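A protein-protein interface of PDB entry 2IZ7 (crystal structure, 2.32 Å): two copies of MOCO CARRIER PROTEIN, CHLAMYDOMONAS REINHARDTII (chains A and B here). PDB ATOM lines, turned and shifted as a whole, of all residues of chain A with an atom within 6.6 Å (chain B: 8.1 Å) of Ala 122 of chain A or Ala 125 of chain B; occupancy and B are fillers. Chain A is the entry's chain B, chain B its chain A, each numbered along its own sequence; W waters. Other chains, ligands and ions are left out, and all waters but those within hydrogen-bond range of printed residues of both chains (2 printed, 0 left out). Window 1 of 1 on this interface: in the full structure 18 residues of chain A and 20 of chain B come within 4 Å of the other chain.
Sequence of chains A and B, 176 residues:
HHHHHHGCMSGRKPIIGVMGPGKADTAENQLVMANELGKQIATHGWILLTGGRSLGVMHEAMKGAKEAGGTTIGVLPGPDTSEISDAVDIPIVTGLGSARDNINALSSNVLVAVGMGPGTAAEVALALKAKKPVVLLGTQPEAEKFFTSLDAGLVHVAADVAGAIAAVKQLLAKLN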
ATOM      1  N   ARG A 100     -15.057  35.182 -16.200  1.00  0.00           N
ATOM      2  CA  ARG A 100     -13.984  34.358 -16.776  1.00  0.00           C
ATOM      3  C   ARG A 100     -13.071  35.485 -17.314  1.00  0.00           C
ATOM      4  O   ARG A 100     -13.574  36.255 -18.147  1.00  0.00           O
ATOM      5  CB  ARG A 100     -14.624  33.531 -17.892  1.00  0.00           C
ATOM      6  CG  ARG A 100     -13.718  32.606 -18.636  1.00  0.00           C
ATOM      7  CD  ARG A 100     -14.290  32.255 -20.019  1.00  0.00           C
ATOM      8  NE  ARG A 100     -13.262  32.060 -21.052  1.00  0.00           N
ATOM      9  CZ  ARG A 100     -13.473  31.474 -22.235  1.00  0.00           C
ATOM     10  NH1 ARG A 100     -14.692  31.007 -22.560  1.00  0.00           N
ATOM     11  NH2 ARG A 100     -12.465  31.361 -23.109  1.00  0.00           N
ATOM     12  N   MET A 116      -3.313  26.580  -9.292  1.00  0.00           N
ATOM     13  CA  MET A 116      -4.691  26.172  -9.528  1.00  0.00           C
ATOM     14  C   MET A 116      -5.650  26.902  -8.656  1.00  0.00           C
ATOM     15  O   MET A 116      -5.312  27.318  -7.562  1.00  0.00           O
ATOM     16  CB  MET A 116      -4.808  24.667  -9.305  1.00  0.00           C
ATOM     17  CG  MET A 116      -6.210  24.068  -9.548  1.00  0.00           C
ATOM     18  SD  MET A 116      -6.798  24.221 -11.215  1.00  0.00           S
ATOM     19  CE  MET A 116      -5.428  23.595 -12.175  1.00  0.00           C
ATOM     20  N   GLY A 117      -6.882  27.004  -9.132  1.00  0.00           N
ATOM     21  CA  GLY A 117      -7.956  27.675  -8.411  1.00  0.00           C
ATOM     22  C   GLY A 117      -9.159  27.633  -9.316  1.00  0.00           C
ATOM     23  O   GLY A 117      -9.083  27.076 -10.406  1.00  0.00           O
ATOM     24  N   PRO A 118     -10.276  28.226  -8.896  1.00  0.00           N
ATOM     25  CA  PRO A 118     -11.491  28.096  -9.745  1.00  0.00           C
ATOM     26  C   PRO A 118     -11.365  28.623 -11.192  1.00  0.00           C
ATOM     27  O   PRO A 118     -11.765  27.912 -12.171  1.00  0.00           O
ATOM     28  CB  PRO A 118     -12.566  28.836  -8.944  1.00  0.00           C
ATOM     29  CG  PRO A 118     -11.985  29.030  -7.563  1.00  0.00           C
ATOM     30  CD  PRO A 118     -10.507  28.994  -7.666  1.00  0.00           C
ATOM     31  N   GLY A 119     -10.786  29.822 -11.336  1.00  0.00           N
ATOM     32  CA  GLY A 119     -10.602  30.415 -12.669  1.00  0.00           C
ATOM     33  C   GLY A 119      -9.745  29.581 -13.564  1.00  0.00           C
ATOM     34  O   GLY A 119     -10.036  29.416 -14.767  1.00  0.00           O
ATOM     35  N   THR A 120      -8.657  29.077 -12.983  1.00  0.00           N
ATOM     36  CA  THR A 120      -7.719  28.232 -13.690  1.00  0.00           C
ATOM     37  C   THR A 120      -8.412  26.923 -14.035  1.00  0.00           C
ATOM     38  O   THR A 120      -8.294  26.446 -15.118  1.00  0.00           O
ATOM     39  CB  THR A 120      -6.446  27.912 -12.809  1.00  0.00           C
ATOM     40  OG1 THR A 120      -5.797  29.112 -12.442  1.00  0.00           O
ATOM     41  CG2 THR A 120      -5.449  27.025 -13.541  1.00  0.00           C
ATOM     42  N   ALA A 121      -9.127  26.349 -13.089  1.00  0.00           N
ATOM     43  CA  ALA A 121      -9.792  25.091 -13.291  1.00  0.00           C
ATOM     44  C   ALA A 121     -10.774  25.187 -14.430  1.00  0.00           C
ATOM     45  O   ALA A 121     -10.892  24.234 -15.173  1.00  0.00           O
ATOM     46  CB  ALA A 121     -10.520  24.648 -12.006  1.00  0.00           C
ATOM     47  N   ALA A 122     -11.444  26.336 -14.591  1.00  0.00           N
ATOM     48  CA  ALA A 122     -12.391  26.540 -15.676  1.00  0.00           C
ATOM     49  C   ALA A 122     -11.712  26.577 -16.989  1.00  0.00           C
ATOM     50  O   ALA A 122     -12.139  25.955 -17.932  1.00  0.00           O
ATOM     51  CB  ALA A 122     -13.172  27.809 -15.488  1.00  0.00           C
ATOM     52  N   GLU A 123     -10.622  27.224 -17.119  1.00  0.00           N
ATOM     53  CA  GLU A 123      -9.886  27.360 -18.360  1.00  0.00           C
ATOM     54  C   GLU A 123      -9.165  26.092 -18.779  1.00  0.00           C
ATOM     55  O   GLU A 123      -9.013  25.823 -19.961  1.00  0.00           O
ATOM     56  CB  GLU A 123      -8.913  28.526 -18.278  1.00  0.00           C
ATOM     57  CG  GLU A 123      -9.536  29.851 -18.651  1.00  0.00           C
ATOM     58  CD  GLU A 123      -9.702  30.749 -17.451  1.00  0.00           C
ATOM     59  OE1 GLU A 123     -10.843  30.925 -16.974  1.00  0.00           O
ATOM     60  OE2 GLU A 123      -8.681  31.279 -16.977  1.00  0.00           O
ATOM     61  N   VAL A 124      -8.637  25.379 -17.766  1.00  0.00           N
ATOM     62  CA  VAL A 124      -8.133  24.028 -18.063  1.00  0.00           C
ATOM     63  C   VAL A 124      -9.274  23.125 -18.562  1.00  0.00           C
ATOM     64  O   VAL A 124      -9.131  22.457 -19.555  1.00  0.00           O
ATOM     65  CB  VAL A 124      -7.414  23.430 -16.789  1.00  0.00           C
ATOM     66  CG1 VAL A 124      -7.166  21.938 -16.909  1.00  0.00           C
ATOM     67  CG2 VAL A 124      -6.118  24.282 -16.453  1.00  0.00           C
ATOM     68  N   ALA A 125     -10.422  23.125 -17.902  1.00  0.00           N
ATOM     69  CA  ALA A 125     -11.537  22.280 -18.354  1.00  0.00           C
ATOM     70  C   ALA A 125     -12.038  22.675 -19.755  1.00  0.00           C
ATOM     71  O   ALA A 125     -12.329  21.824 -20.577  1.00  0.00           O
ATOM     72  CB  ALA A 125     -12.650  22.327 -17.375  1.00  0.00           C
ATOM     73  N   LEU A 126     -12.109  23.966 -20.041  1.00  0.00           N
ATOM     74  CA  LEU A 126     -12.496  24.448 -21.368  1.00  0.00           C
ATOM     75  C   LEU A 126     -11.520  24.112 -22.495  1.00  0.00           C
ATOM     76  O   LEU A 126     -11.934  23.820 -23.630  1.00  0.00           O
ATOM     77  CB  LEU A 126     -12.724  25.952 -21.348  1.00  0.00           C
ATOM     78  CG  LEU A 126     -13.887  26.478 -20.500  1.00  0.00           C
ATOM     79  CD1 LEU A 126     -13.832  28.025 -20.444  1.00  0.00           C
ATOM     80  CD2 LEU A 126     -15.199  25.980 -21.011  1.00  0.00           C
ATOM     81  N   ALA A 127     -10.229  24.150 -22.214  1.00  0.00           N
ATOM     82  CA  ALA A 127      -9.234  23.712 -23.212  1.00  0.00           C
ATOM     83  C   ALA A 127      -9.464  22.260 -23.579  1.00  0.00           C
ATOM     84  O   ALA A 127      -9.499  21.927 -24.732  1.00  0.00           O
ATOM     85  CB  ALA A 127      -7.832  23.899 -22.680  1.00  0.00           C
ATOM     86  N   PHE A 147      -8.221  16.192 -13.617  1.00  0.00           N
ATOM     87  CA  PHE A 147      -8.181  16.566 -15.022  1.00  0.00           C
ATOM     88  C   PHE A 147      -7.817  15.389 -15.868  1.00  0.00           C
ATOM     89  O   PHE A 147      -8.437  15.142 -16.898  1.00  0.00           O
ATOM     90  CB  PHE A 147      -7.226  17.745 -15.244  1.00  0.00           C
ATOM     91  CG  PHE A 147      -7.766  19.015 -14.704  1.00  0.00           C
ATOM     92  CD1 PHE A 147      -8.965  19.531 -15.212  1.00  0.00           C
ATOM     93  CD2 PHE A 147      -7.137  19.674 -13.650  1.00  0.00           C
ATOM     94  CE1 PHE A 147      -9.523  20.694 -14.697  1.00  0.00           C
ATOM     95  CE2 PHE A 147      -7.694  20.851 -13.110  1.00  0.00           C
ATOM     96  CZ  PHE A 147      -8.908  21.346 -13.641  1.00  0.00           C
ATOM     97  N   ALA B  99     -18.191  26.519 -27.091  1.00  0.00           N
ATOM     98  CA  ALA B  99     -17.161  26.579 -26.062  1.00  0.00           C
ATOM     99  C   ALA B  99     -17.737  26.255 -24.686  1.00  0.00           C
ATOM    100  O   ALA B  99     -17.234  25.379 -23.983  1.00  0.00           O
ATOM    101  CB  ALA B  99     -16.500  27.948 -26.053  1.00  0.00           C
ATOM    102  N   ARG B 100     -18.775  26.807 -24.403  1.00  0.00           N
ATOM    103  CA  ARG B 100     -19.556  26.373 -23.250  1.00  0.00           C
ATOM    104  C   ARG B 100     -20.966  25.963 -23.662  1.00  0.00           C
ATOM    105  O   ARG B 100     -21.208  25.610 -24.817  1.00  0.00           O
ATOM    106  CB  ARG B 100     -19.618  27.482 -22.198  1.00  0.00           C
ATOM    107  CG  ARG B 100     -18.268  28.095 -21.861  1.00  0.00           C
ATOM    108  CD  ARG B 100     -18.248  29.615 -21.907  1.00  0.00           C
ATOM    109  NE  ARG B 100     -17.995  30.119 -23.253  1.00  0.00           N
ATOM    110  CZ  ARG B 100     -18.204  31.373 -23.630  1.00  0.00           C
ATOM    111  NH1 ARG B 100     -18.670  32.260 -22.762  1.00  0.00           N
ATOM    112  NH2 ARG B 100     -17.945  31.743 -24.878  1.00  0.00           N
ATOM    113  N   LEU B 111     -26.456  25.876  -8.227  1.00  0.00           N
ATOM    114  CA  LEU B 111     -26.146  25.053  -9.365  1.00  0.00           C
ATOM    115  C   LEU B 111     -26.124  23.648  -8.916  1.00  0.00           C
ATOM    116  O   LEU B 111     -25.547  23.367  -7.880  1.00  0.00           O
ATOM    117  CB  LEU B 111     -24.740  25.321  -9.801  1.00  0.00           C
ATOM    118  CG  LEU B 111     -24.449  26.464 -10.688  1.00  0.00           C
ATOM    119  CD1 LEU B 111     -23.308  26.058 -11.650  1.00  0.00           C
ATOM    120  CD2 LEU B 111     -25.649  26.893 -11.429  1.00  0.00           C
ATOM    121  N   MET B 116     -20.479  14.541 -14.867  1.00  0.00           N
ATOM    122  CA  MET B 116     -19.266  15.356 -15.004  1.00  0.00           C
ATOM    123  C   MET B 116     -18.574  15.028 -16.305  1.00  0.00           C
ATOM    124  O   MET B 116     -18.687  13.912 -16.798  1.00  0.00           O
ATOM    125  CB  MET B 116     -18.326  15.105 -13.836  1.00  0.00           C
ATOM    126  CG  MET B 116     -17.087  15.972 -13.774  1.00  0.00           C
ATOM    127  SD  MET B 116     -17.330  17.695 -13.565  1.00  0.00           S
ATOM    128  CE  MET B 116     -18.445  17.734 -12.175  1.00  0.00           C
ATOM    129  N   PRO B 118     -15.744  17.650 -19.200  1.00  0.00           N
ATOM    130  CA  PRO B 118     -15.087  18.970 -19.365  1.00  0.00           C
ATOM    131  C   PRO B 118     -15.990  20.192 -19.278  1.00  0.00           C
ATOM    132  O   PRO B 118     -15.717  21.083 -18.495  1.00  0.00           O
ATOM    133  CB  PRO B 118     -14.419  18.844 -20.722  1.00  0.00           C
ATOM    134  CG  PRO B 118     -14.103  17.399 -20.823  1.00  0.00           C
ATOM    135  CD  PRO B 118     -15.269  16.678 -20.201  1.00  0.00           C
ATOM    136  N   GLY B 119     -17.074  20.234 -20.052  1.00  0.00           N
ATOM    137  CA  GLY B 119     -18.017  21.334 -19.969  1.00  0.00           C
ATOM    138  C   GLY B 119     -18.603  21.584 -18.609  1.00  0.00           C
ATOM    139  O   GLY B 119     -18.690  22.725 -18.144  1.00  0.00           O
ATOM    140  N   THR B 120     -19.009  20.516 -17.938  1.00  0.00           N
ATOM    141  CA  THR B 120     -19.563  20.615 -16.625  1.00  0.00           C
ATOM    142  C   THR B 120     -18.545  21.096 -15.588  1.00  0.00           C
ATOM    143  O   THR B 120     -18.854  21.925 -14.751  1.00  0.00           O
ATOM    144  CB  THR B 120     -20.073  19.239 -16.194  1.00  0.00           C
ATOM    145  OG1 THR B 120     -20.910  18.722 -17.210  1.00  0.00           O
ATOM    146  CG2 THR B 120     -20.841  19.323 -14.948  1.00  0.00           C
ATOM    147  N   ALA B 121     -17.336  20.555 -15.650  1.00  0.00           N
ATOM    148  CA  ALA B 121     -16.224  20.955 -14.789  1.00  0.00           C
ATOM    149  C   ALA B 121     -15.965  22.488 -14.879  1.00  0.00           C
ATOM    150  O   ALA B 121     -15.845  23.151 -13.842  1.00  0.00           O
ATOM    151  CB  ALA B 121     -14.968  20.131 -15.183  1.00  0.00           C
ATOM    152  N   ALA B 122     -15.956  23.027 -16.104  1.00  0.00           N
ATOM    153  CA  ALA B 122     -15.764  24.439 -16.363  1.00  0.00           C
ATOM    154  C   ALA B 122     -16.814  25.306 -15.754  1.00  0.00           C
ATOM    155  O   ALA B 122     -16.513  26.314 -15.133  1.00  0.00           O
ATOM    156  CB  ALA B 122     -15.690  24.688 -17.852  1.00  0.00           C
ATOM    157  N   GLU B 123     -18.074  24.912 -15.886  1.00  0.00           N
ATOM    158  CA  GLU B 123     -19.172  25.646 -15.253  1.00  0.00           C
ATOM    159  C   GLU B 123     -19.235  25.534 -13.790  1.00  0.00           C
ATOM    160  O   GLU B 123     -19.601  26.484 -13.128  1.00  0.00           O
ATOM    161  CB  GLU B 123     -20.484  25.161 -15.813  1.00  0.00           C
ATOM    162  CG  GLU B 123     -20.552  25.483 -17.271  1.00  0.00           C
ATOM    163  CD  GLU B 123     -20.995  26.900 -17.496  1.00  0.00           C
ATOM    164  OE1 GLU B 123     -20.193  27.709 -18.084  1.00  0.00           O
ATOM    165  OE2 GLU B 123     -22.159  27.181 -17.098  1.00  0.00           O
ATOM    166  N   VAL B 124     -18.923  24.374 -13.250  1.00  0.00           N
ATOM    167  CA  VAL B 124     -18.767  24.265 -11.784  1.00  0.00           C
ATOM    168  C   VAL B 124     -17.667  25.231 -11.231  1.00  0.00           C
ATOM    169  O   VAL B 124     -17.868  25.976 -10.265  1.00  0.00           O
ATOM    170  CB  VAL B 124     -18.537  22.809 -11.340  1.00  0.00           C
ATOM    171  CG1 VAL B 124     -18.181  22.753  -9.861  1.00  0.00           C
ATOM    172  CG2 VAL B 124     -19.822  21.941 -11.617  1.00  0.00           C
ATOM    173  N   ALA B 125     -16.520  25.231 -11.886  1.00  0.00           N
ATOM    174  CA  ALA B 125     -15.409  26.088 -11.472  1.00  0.00           C
ATOM    175  C   ALA B 125     -15.806  27.579 -11.516  1.00  0.00           C
ATOM    176  O   ALA B 125     -15.543  28.343 -10.582  1.00  0.00           O
ATOM    177  CB  ALA B 125     -14.261  25.825 -12.349  1.00  0.00           C
ATOM    178  N   LEU B 126     -16.457  27.968 -12.613  1.00  0.00           N
ATOM    179  CA  LEU B 126     -16.918  29.325 -12.851  1.00  0.00           C
ATOM    180  C   LEU B 126     -17.956  29.813 -11.819  1.00  0.00           C
ATOM    181  O   LEU B 126     -17.988  30.979 -11.463  1.00  0.00           O
ATOM    182  CB  LEU B 126     -17.551  29.418 -14.242  1.00  0.00           C
ATOM    183  CG  LEU B 126     -16.564  29.433 -15.384  1.00  0.00           C
ATOM    184  CD1 LEU B 126     -17.334  29.653 -16.665  1.00  0.00           C
ATOM    185  CD2 LEU B 126     -15.521  30.559 -15.186  1.00  0.00           C
ATOM    186  N   ALA B 127     -18.795  28.902 -11.385  1.00  0.00           N
ATOM    187  CA  ALA B 127     -19.767  29.141 -10.330  1.00  0.00           C
ATOM    188  C   ALA B 127     -19.057  29.222  -8.975  1.00  0.00           C
ATOM    189  O   ALA B 127     -19.358  30.072  -8.154  1.00  0.00           O
ATOM    190  CB  ALA B 127     -20.826  28.048 -10.359  1.00  0.00           C
ATOM    191  N   LEU B 128     -18.053  28.398  -8.743  1.00  0.00           N
ATOM    192  CA  LEU B 128     -17.248  28.589  -7.537  1.00  0.00           C
ATOM    193  C   LEU B 128     -16.519  29.931  -7.547  1.00  0.00           C
ATOM    194  O   LEU B 128     -16.470  30.657  -6.547  1.00  0.00           O
ATOM    195  CB  LEU B 128     -16.275  27.408  -7.368  1.00  0.00           C
ATOM    196  CG  LEU B 128     -17.116  26.134  -7.083  1.00  0.00           C
ATOM    197  CD1 LEU B 128     -16.254  24.878  -7.117  1.00  0.00           C
ATOM    198  CD2 LEU B 128     -17.871  26.283  -5.746  1.00  0.00           C
ATOM    199  N   LYS B 129     -15.947  30.265  -8.692  1.00  0.00           N
ATOM    200  CA  LYS B 129     -15.351  31.553  -8.861  1.00  0.00           C
ATOM    201  C   LYS B 129     -16.339  32.709  -8.634  1.00  0.00           C
ATOM    202  O   LYS B 129     -15.959  33.743  -8.142  1.00  0.00           O
ATOM    203  CB  LYS B 129     -14.757  31.630 -10.265  1.00  0.00           C
ATOM    204  CG  LYS B 129     -13.962  32.850 -10.475  1.00  0.00           C
ATOM    205  CD  LYS B 129     -13.491  32.949 -11.869  1.00  0.00           C
ATOM    206  CE  LYS B 129     -12.909  34.351 -12.095  1.00  0.00           C
ATOM    207  NZ  LYS B 129     -12.357  34.428 -13.446  1.00  0.00           N
ATOM    208  N   ALA B 130     -17.589  32.524  -9.042  1.00  0.00           N
ATOM    209  CA  ALA B 130     -18.677  33.475  -8.818  1.00  0.00           C
ATOM    210  C   ALA B 130     -19.207  33.445  -7.381  1.00  0.00           C
ATOM    211  O   ALA B 130     -20.131  34.193  -7.061  1.00  0.00           O
ATOM    212  CB  ALA B 130     -19.847  33.165  -9.781  1.00  0.00           C
ATOM    213  N   LYS B 131     -18.629  32.579  -6.546  1.00  0.00           N
ATOM    214  CA  LYS B 131     -19.013  32.374  -5.141  1.00  0.00           C
ATOM    215  C   LYS B 131     -20.435  31.892  -4.995  1.00  0.00           C
ATOM    216  O   LYS B 131     -21.153  32.245  -4.063  1.00  0.00           O
ATOM    217  CB  LYS B 131     -18.736  33.607  -4.274  1.00  0.00           C
ATOM    218  CG  LYS B 131     -17.309  34.110  -4.443  1.00  0.00           C
ATOM    219  CD  LYS B 131     -16.291  33.148  -3.854  1.00  0.00           C
ATOM    220  CE  LYS B 131     -14.918  33.814  -3.665  1.00  0.00           C
ATOM    221  NZ  LYS B 131     -14.079  33.183  -2.554  1.00  0.00           N
ATOM    222  N   LYS B 132     -20.825  31.044  -5.925  1.00  0.00           N
ATOM    223  CA  LYS B 132     -22.135  30.434  -5.886  1.00  0.00           C
ATOM    224  C   LYS B 132     -21.957  29.007  -5.403  1.00  0.00           C
ATOM    225  O   LYS B 132     -20.915  28.414  -5.672  1.00  0.00           O
ATOM    226  CB  LYS B 132     -22.839  30.548  -7.245  1.00  0.00           C
ATOM    227  CG  LYS B 132     -23.163  32.005  -7.536  1.00  0.00           C
ATOM    228  CD  LYS B 132     -23.948  32.195  -8.836  1.00  0.00           C
ATOM    229  CE  LYS B 132     -24.830  33.460  -8.834  1.00  0.00           C
ATOM    230  NZ  LYS B 132     -25.855  33.386  -7.768  1.00  0.00           N
ATOM    231  N   VAL B 134     -22.661  24.949  -5.194  1.00  0.00           N
ATOM    232  CA  VAL B 134     -22.796  23.945  -6.220  1.00  0.00           C
ATOM    233  C   VAL B 134     -23.023  22.679  -5.483  1.00  0.00           C
ATOM    234  O   VAL B 134     -22.355  22.397  -4.486  1.00  0.00           O
ATOM    235  CB  VAL B 134     -21.555  23.733  -7.091  1.00  0.00           C
ATOM    236  CG1 VAL B 134     -21.791  22.546  -8.005  1.00  0.00           C
ATOM    237  CG2 VAL B 134     -21.178  24.954  -7.926  1.00  0.00           C
ATOM    238  N   LEU B 136     -23.051  18.631  -6.165  1.00  0.00           N
ATOM    239  CA  LEU B 136     -22.441  17.682  -7.032  1.00  0.00           C
ATOM    240  C   LEU B 136     -23.177  16.363  -6.831  1.00  0.00           C
ATOM    241  O   LEU B 136     -23.112  15.775  -5.771  1.00  0.00           O
ATOM    242  CB  LEU B 136     -20.980  17.540  -6.606  1.00  0.00           C
ATOM    243  CG  LEU B 136     -20.004  18.701  -6.822  1.00  0.00           C
ATOM    244  CD1 LEU B 136     -18.560  18.198  -6.452  1.00  0.00           C
ATOM    245  CD2 LEU B 136     -19.964  19.168  -8.203  1.00  0.00           C
ATOM    246  N   PHE B 146     -11.583  17.450  -5.696  1.00  0.00           N
ATOM    247  CA  PHE B 146     -11.064  18.575  -6.403  1.00  0.00           C
ATOM    248  C   PHE B 146     -11.908  19.800  -6.156  1.00  0.00           C
ATOM    249  O   PHE B 146     -11.359  20.829  -5.783  1.00  0.00           O
ATOM    250  CB  PHE B 146     -10.974  18.337  -7.896  1.00  0.00           C
ATOM    251  CG  PHE B 146     -10.409  19.510  -8.618  1.00  0.00           C
ATOM    252  CD1 PHE B 146      -9.103  19.925  -8.369  1.00  0.00           C
ATOM    253  CD2 PHE B 146     -11.187  20.245  -9.482  1.00  0.00           C
ATOM    254  CE1 PHE B 146      -8.587  21.042  -8.999  1.00  0.00           C
ATOM    255  CE2 PHE B 146     -10.674  21.346 -10.125  1.00  0.00           C
ATOM    256  CZ  PHE B 146      -9.370  21.750  -9.892  1.00  0.00           C
ATOM    257  N   PHE B 147     -13.218  19.692  -6.314  1.00  0.00           N
ATOM    258  CA  PHE B 147     -14.053  20.884  -6.196  1.00  0.00           C
ATOM    259  C   PHE B 147     -14.136  21.330  -4.780  1.00  0.00           C
ATOM    260  O   PHE B 147     -14.062  22.526  -4.508  1.00  0.00           O
ATOM    261  CB  PHE B 147     -15.436  20.702  -6.875  1.00  0.00           C
ATOM    262  CG  PHE B 147     -15.339  20.653  -8.408  1.00  0.00           C
ATOM    263  CD1 PHE B 147     -15.557  19.491  -9.112  1.00  0.00           C
ATOM    264  CD2 PHE B 147     -14.955  21.784  -9.129  1.00  0.00           C
ATOM    265  CE1 PHE B 147     -15.412  19.454 -10.507  1.00  0.00           C
ATOM    266  CE2 PHE B 147     -14.834  21.731 -10.511  1.00  0.00           C
ATOM    267  CZ  PHE B 147     -15.053  20.557 -11.176  1.00  0.00           C
ATOM    268  N   LEU B 150     -11.306  23.334  -4.110  1.00  0.00           N
ATOM    269  CA  LEU B 150     -11.385  24.717  -4.604  1.00  0.00           C
ATOM    270  C   LEU B 150     -12.076  25.665  -3.617  1.00  0.00           C
ATOM    271  O   LEU B 150     -11.641  26.801  -3.459  1.00  0.00           O
ATOM    272  CB  LEU B 150     -12.026  24.822  -6.005  1.00  0.00           C
ATOM    273  CG  LEU B 150     -11.246  24.152  -7.155  1.00  0.00           C
ATOM    274  CD1 LEU B 150     -12.011  24.284  -8.466  1.00  0.00           C
ATOM    275  CD2 LEU B 150      -9.842  24.716  -7.268  1.00  0.00           C
ATOM    276  N   ASP B 151     -13.139  25.186  -2.979  1.00  0.00           N
ATOM    277  CA  ASP B 151     -13.963  25.973  -2.047  1.00  0.00           C
ATOM    278  C   ASP B 151     -14.832  25.013  -1.252  1.00  0.00           C
ATOM    279  O   ASP B 151     -15.880  24.626  -1.678  1.00  0.00           O
ATOM    280  CB  ASP B 151     -14.855  26.975  -2.809  1.00  0.00           C
ATOM    281  CG  ASP B 151     -15.384  28.082  -1.906  1.00  0.00           C
ATOM    282  OD1 ASP B 151     -15.943  27.734  -0.843  1.00  0.00           O
ATOM    283  OD2 ASP B 151     -15.214  29.282  -2.236  1.00  0.00           O
ATOM    284  N   LEU B 154     -18.469  26.104  -0.450  1.00  0.00           N
ATOM    285  CA  LEU B 154     -19.469  26.256  -1.533  1.00  0.00           C
ATOM    286  C   LEU B 154     -19.911  24.976  -2.201  1.00  0.00           C
ATOM    287  O   LEU B 154     -20.883  25.014  -2.902  1.00  0.00           O
ATOM    288  CB  LEU B 154     -18.939  27.203  -2.647  1.00  0.00           C
ATOM    289  CG  LEU B 154     -18.757  28.661  -2.217  1.00  0.00           C
ATOM    290  CD1 LEU B 154     -18.168  29.477  -3.401  1.00  0.00           C
ATOM    291  CD2 LEU B 154     -20.018  29.296  -1.670  1.00  0.00           C
HETATM  292  O   HOH W   1     -13.962  24.806 -24.951  1.00  0.00           O
HETATM  293  O   HOH W   2     -12.815  22.406 -13.629  1.00  0.00           O
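The guanidinium group (NE) of Arg 100 of chain B sits close to the guanidinium group (NH1) of Arg 100 of chain A (3.5 Å).
The side-chain sulfur (SD) of Met 116 of chain A is in hydrogen-bond range of the backbone NH (N) of Ala 121 of chain A. SD of Met 116 of chain B lies within hydrogen-bond range of N of Ala 121 of chain B (3.5 Å).
Among the printed residues, pairs that only touch across the chains: Arg 100 of chain A with Lys 129 of chain B, Met 116 of chain A with Phe 146 of chain B, Gly 117 of chain A with Leu 150 of chain B, Pro 118 of chain A with Ala 125 of chain B, Pro 118 of chain A with Lys 129 of chain B, Pro 118 of chain A with Leu 150 of chain B, Gly 119 of chain A with Lys 129 of chain B, Ala 121 of chain A with Ala 125 of chain B, Ala 121 of chain A with Phe 146 of chain B, Ala 121 of chain A with Leu 150 of chain B, Ala 122 of chain A with Ala 122 of chain B, Ala 122 of chain A with Ala 125 of chain B, Ala 122 of chain A with Leu 126 of chain B, Ala 125 of chain A with Pro 118 of chain B, Ala 125 of chain A with Ala 121 of chain B, Ala 125 of chain A with Ala 122 of chain B, Leu 126 of chain A with Ala 99 of chain B, Leu 126 of chain A with Arg 100 of chain B, Leu 126 of chain A with Ala 122 of chain B and Phe 147 of chain A with Phe 146 of chain B.
Of the printed residues of chain B, Ala 121 of chain A touches Ala 125 (3.9 Å), Phe 146 (3.8 Å) and Leu 150 (3.9 Å). Of chain B, only Ala 122, Ala 125 and Leu 126 come within 4 Å of Ala 122 of chain A. Printed residues of chain B within 4 Å of Leu 126 of chain A: Ala 99 (3.7 Å), Arg 100 (3.8 Å) and Ala 122 (3.4 Å). Leu 111 of chain B touches none of the printed residues of chain A. Val 124 of chain B touches none of the printed residues of chain A. Printed residues of chain A within 4 Å of Ala 125 of chain B: Pro 118 (3.3 Å), Ala 121 (3.9 Å) and Ala 122 (3.6 Å). Of the printed residues of chain A, Lys 129 of chain B touches Arg 100, Pro 118 and Gly 119. The nearest residue of chain A that does not touch Ala 125 of chain B is Gly 119 of chain A (5.0 Å). The nearest printed residue of chain B that does not touch Phe 147 of chain A is Ala 121 of chain B (5.5 Å).
Printed residues of chain A that touch a printed residue of chain B: Arg 100, Met 116, Gly 117, Pro 118, Gly 119, Ala 121, Ala 122, Ala 125, Leu 126 and Phe 147. Hydrophobic or aromatic side chains of chain A within 4 Å of the printed part of chain B: Met 116, Pro 118, Ala 121, Ala 122, Ala 125, Leu 126 and Phe 147. Of the 26 printed residues of chain B, 10 touch a printed residue of chain A. Printed residues of chain B that touch a printed residue of chain A: Ala 99, Arg 100, Pro 118, Ala 121, Ala 122, Ala 125, Leu 126, Lys 129, Phe 146 and Leu 150. Hydrophobic or aromatic side chains of chain B within 4 Å of the printed part of chain A: Pro 118, Ala 121, Ala 122, Ala 125, Leu 126, Phe 146 and Leu 150. Among the printed residues, 21 pairs touch across the chains.
Arg 100 of chain A touches its own counterpart, Arg 100 of chain B. Pro 118 of chain A touches Ala 125 of chain B, and with the chains exchanged Ala 125 of chain A touches Pro 118 of chain B. Ala 121 of chain A touches Ala 125 of chain B, and with the chains exchanged Ala 125 of chain A touches Ala 121 of chain B. Ala 122 of chain A touches Leu 126 of chain B, and with the chains exchanged Leu 126 of chain A touches Ala 122 of chain B. Positions printed for both chains: 100, 116, 118, 119, 120, 121, 122, 123, 124, 125, 126, 127 and 147. Of the 21 pairs that touch across the chains among the printed residues, 10 have their exchanged pair printed and touching as well.
Water W1 bridges O of Leu 126 of chain A (2.6 Å) and O of Ala 99 of chain B (3.5 Å). Water W2 bridges the backbone carbonyl oxygen of Ala 121 of chain A and the backbone carbonyl oxygen of Ala 121 of chain B.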
